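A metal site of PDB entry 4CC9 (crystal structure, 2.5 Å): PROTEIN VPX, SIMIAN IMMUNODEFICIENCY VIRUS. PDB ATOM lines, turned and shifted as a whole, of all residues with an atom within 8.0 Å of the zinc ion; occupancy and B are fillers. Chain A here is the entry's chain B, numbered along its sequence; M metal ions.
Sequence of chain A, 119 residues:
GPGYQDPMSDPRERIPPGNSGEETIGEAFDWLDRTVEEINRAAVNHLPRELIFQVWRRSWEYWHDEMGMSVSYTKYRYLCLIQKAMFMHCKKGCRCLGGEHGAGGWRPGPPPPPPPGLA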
ATOM      1  N   ALA A  42     -21.128 -15.639 -16.154  1.00  0.00           N
ATOM      2  CA  ALA A  42     -20.681 -16.361 -17.351  1.00  0.00           C
ATOM      3  C   ALA A  42     -21.149 -17.820 -17.326  1.00  0.00           C
ATOM      4  O   ALA A  42     -21.649 -18.351 -18.341  1.00  0.00           O
ATOM      5  CB  ALA A  42     -19.175 -16.299 -17.494  1.00  0.00           C
ATOM      6  N   ALA A  43     -21.002 -18.461 -16.172  1.00  0.00           N
ATOM      7  CA  ALA A  43     -21.265 -19.901 -16.059  1.00  0.00           C
ATOM      8  C   ALA A  43     -22.719 -20.302 -16.264  1.00  0.00           C
ATOM      9  O   ALA A  43     -22.996 -21.433 -16.653  1.00  0.00           O
ATOM     10  CB  ALA A  43     -20.756 -20.437 -14.729  1.00  0.00           C
ATOM     11  N   ASN A  45     -24.580 -19.429 -18.546  1.00  0.00           N
ATOM     12  CA  ASN A  45     -24.805 -19.651 -19.982  1.00  0.00           C
ATOM     13  C   ASN A  45     -24.197 -20.949 -20.501  1.00  0.00           C
ATOM     14  O   ASN A  45     -24.285 -21.235 -21.694  1.00  0.00           O
ATOM     15  CB  ASN A  45     -24.228 -18.477 -20.800  1.00  0.00           C
ATOM     16  CG  ASN A  45     -24.863 -17.146 -20.448  1.00  0.00           C
ATOM     17  OD1 ASN A  45     -26.027 -17.090 -20.045  1.00  0.00           O
ATOM     18  ND2 ASN A  45     -24.105 -16.066 -20.616  1.00  0.00           N
ATOM     19  N   HIS A  46     -23.588 -21.740 -19.620  1.00  0.00           N
ATOM     20  CA  HIS A  46     -22.917 -22.979 -20.047  1.00  0.00           C
ATOM     21  C   HIS A  46     -23.265 -24.158 -19.156  1.00  0.00           C
ATOM     22  O   HIS A  46     -23.374 -25.285 -19.628  1.00  0.00           O
ATOM     23  CB  HIS A  46     -21.395 -22.792 -20.032  1.00  0.00           C
ATOM     24  CG  HIS A  46     -20.898 -21.742 -20.970  1.00  0.00           C
ATOM     25  ND1 HIS A  46     -20.570 -22.017 -22.285  1.00  0.00           N
ATOM     26  CD2 HIS A  46     -20.662 -20.427 -20.787  1.00  0.00           C
ATOM     27  CE1 HIS A  46     -20.155 -20.912 -22.868  1.00  0.00           C
ATOM     28  NE2 HIS A  46     -20.209 -19.930 -21.991  1.00  0.00           N
ATOM     29  N   LEU A  47     -23.408 -23.898 -17.858  1.00  0.00           N
ATOM     30  CA  LEU A  47     -23.625 -24.971 -16.895  1.00  0.00           C
ATOM     31  C   LEU A  47     -25.047 -24.862 -16.366  1.00  0.00           C
ATOM     32  O   LEU A  47     -25.611 -23.775 -16.354  1.00  0.00           O
ATOM     33  CB  LEU A  47     -22.617 -24.858 -15.743  1.00  0.00           C
ATOM     34  CG  LEU A  47     -21.152 -24.694 -16.147  1.00  0.00           C
ATOM     35  CD1 LEU A  47     -20.268 -24.537 -14.933  1.00  0.00           C
ATOM     36  CD2 LEU A  47     -20.671 -25.868 -16.986  1.00  0.00           C
ATOM     37  N   MET A  86     -15.554 -24.984 -15.491  1.00  0.00           N
ATOM     38  CA  MET A  86     -15.582 -24.268 -16.773  1.00  0.00           C
ATOM     39  C   MET A  86     -14.517 -24.814 -17.708  1.00  0.00           C
ATOM     40  O   MET A  86     -14.772 -24.963 -18.906  1.00  0.00           O
ATOM     41  CB  MET A  86     -15.390 -22.762 -16.572  1.00  0.00           C
ATOM     42  CG  MET A  86     -16.597 -22.079 -15.979  1.00  0.00           C
ATOM     43  SD  MET A  86     -17.992 -22.108 -17.118  1.00  0.00           S
ATOM     44  CE  MET A  86     -17.386 -21.016 -18.407  1.00  0.00           C
ATOM     45  N   HIS A  89     -15.805 -27.947 -19.223  1.00  0.00           N
ATOM     46  CA  HIS A  89     -16.847 -27.683 -20.215  1.00  0.00           C
ATOM     47  C   HIS A  89     -16.262 -27.226 -21.553  1.00  0.00           C
ATOM     48  O   HIS A  89     -16.693 -27.678 -22.609  1.00  0.00           O
ATOM     49  CB  HIS A  89     -17.851 -26.645 -19.700  1.00  0.00           C
ATOM     50  CG  HIS A  89     -18.862 -26.231 -20.717  1.00  0.00           C
ATOM     51  ND1 HIS A  89     -20.017 -26.950 -20.963  1.00  0.00           N
ATOM     52  CD2 HIS A  89     -18.910 -25.159 -21.534  1.00  0.00           C
ATOM     53  CE1 HIS A  89     -20.720 -26.345 -21.895  1.00  0.00           C
ATOM     54  NE2 HIS A  89     -20.074 -25.249 -22.268  1.00  0.00           N
ATOM     55  N   CYS A  90     -15.272 -26.348 -21.498  1.00  0.00           N
ATOM     56  CA  CYS A  90     -14.730 -25.775 -22.729  1.00  0.00           C
ATOM     57  C   CYS A  90     -13.793 -26.708 -23.483  1.00  0.00           C
ATOM     58  O   CYS A  90     -13.717 -26.661 -24.710  1.00  0.00           O
ATOM     59  CB  CYS A  90     -14.085 -24.420 -22.437  1.00  0.00           C
ATOM     60  SG  CYS A  90     -15.316 -23.144 -21.977  1.00  0.00           S
ATOM     61  N   GLY A  93     -15.588 -28.769 -25.883  1.00  0.00           N
ATOM     62  CA  GLY A  93     -16.068 -28.059 -27.041  1.00  0.00           C
ATOM     63  C   GLY A  93     -17.439 -27.504 -26.757  1.00  0.00           C
ATOM     64  O   GLY A  93     -18.340 -28.224 -26.288  1.00  0.00           O
ATOM     65  N   CYS A  94     -17.609 -26.220 -27.058  1.00  0.00           N
ATOM     66  CA  CYS A  94     -18.778 -25.486 -26.608  1.00  0.00           C
ATOM     67  C   CYS A  94     -19.522 -24.781 -27.734  1.00  0.00           C
ATOM     68  O   CYS A  94     -18.995 -23.852 -28.355  1.00  0.00           O
ATOM     69  CB  CYS A  94     -18.343 -24.475 -25.541  1.00  0.00           C
ATOM     70  SG  CYS A  94     -19.541 -23.198 -25.174  1.00  0.00           S
ATOM     71  N   ARG A  95     -20.737 -25.244 -27.997  1.00  0.00           N
ATOM     72  CA  ARG A  95     -21.651 -24.560 -28.921  1.00  0.00           C
ATOM     73  C   ARG A  95     -22.863 -24.009 -28.151  1.00  0.00           C
ATOM     74  O   ARG A  95     -24.007 -24.221 -28.543  1.00  0.00           O
ATOM     75  CB  ARG A  95     -22.111 -25.521 -30.027  1.00  0.00           C
ATOM     76  N   CYS A  96     -22.585 -23.299 -27.063  1.00  0.00           N
ATOM     77  CA  CYS A  96     -23.641 -22.751 -26.222  1.00  0.00           C
ATOM     78  C   CYS A  96     -24.170 -21.414 -26.749  1.00  0.00           C
ATOM     79  O   CYS A  96     -23.407 -20.593 -27.258  1.00  0.00           O
ATOM     80  CB  CYS A  96     -23.157 -22.586 -24.776  1.00  0.00           C
ATOM     81  SG  CYS A  96     -23.085 -24.132 -23.838  1.00  0.00           S
ATOM     82  N   LEU A  97     -25.479 -21.213 -26.621  1.00  0.00           N
ATOM     83  CA  LEU A  97     -26.110 -19.970 -27.044  1.00  0.00           C
ATOM     84  C   LEU A  97     -25.727 -18.805 -26.135  1.00  0.00           C
ATOM     85  O   LEU A  97     -25.318 -17.745 -26.624  1.00  0.00           O
ATOM     86  CB  LEU A  97     -27.631 -20.135 -27.066  1.00  0.00           C
HETATM   87 ZN    ZN M   1     -20.871 -23.678 -23.338  1.00  0.00          ZN
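SG of Cys 96 lies close to O of Asn 45 (3.8 Å).
Four residues have an atom within 4 Å of the zinc ion: His 46, His 89, Cys 94 and Cys 96. The nearest printed residue that does not touch the zinc ion is Asn 45 (4.5 Å).
The zinc ion is bound by a ring nitrogen (ND1) of His 46 (2.0 Å), a ring nitrogen (NE2) of His 89 (2.1 Å), the side-chain sulfur of Cys 96 (2.3 Å) and the side-chain sulfur of Cys 94 (2.3 Å).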
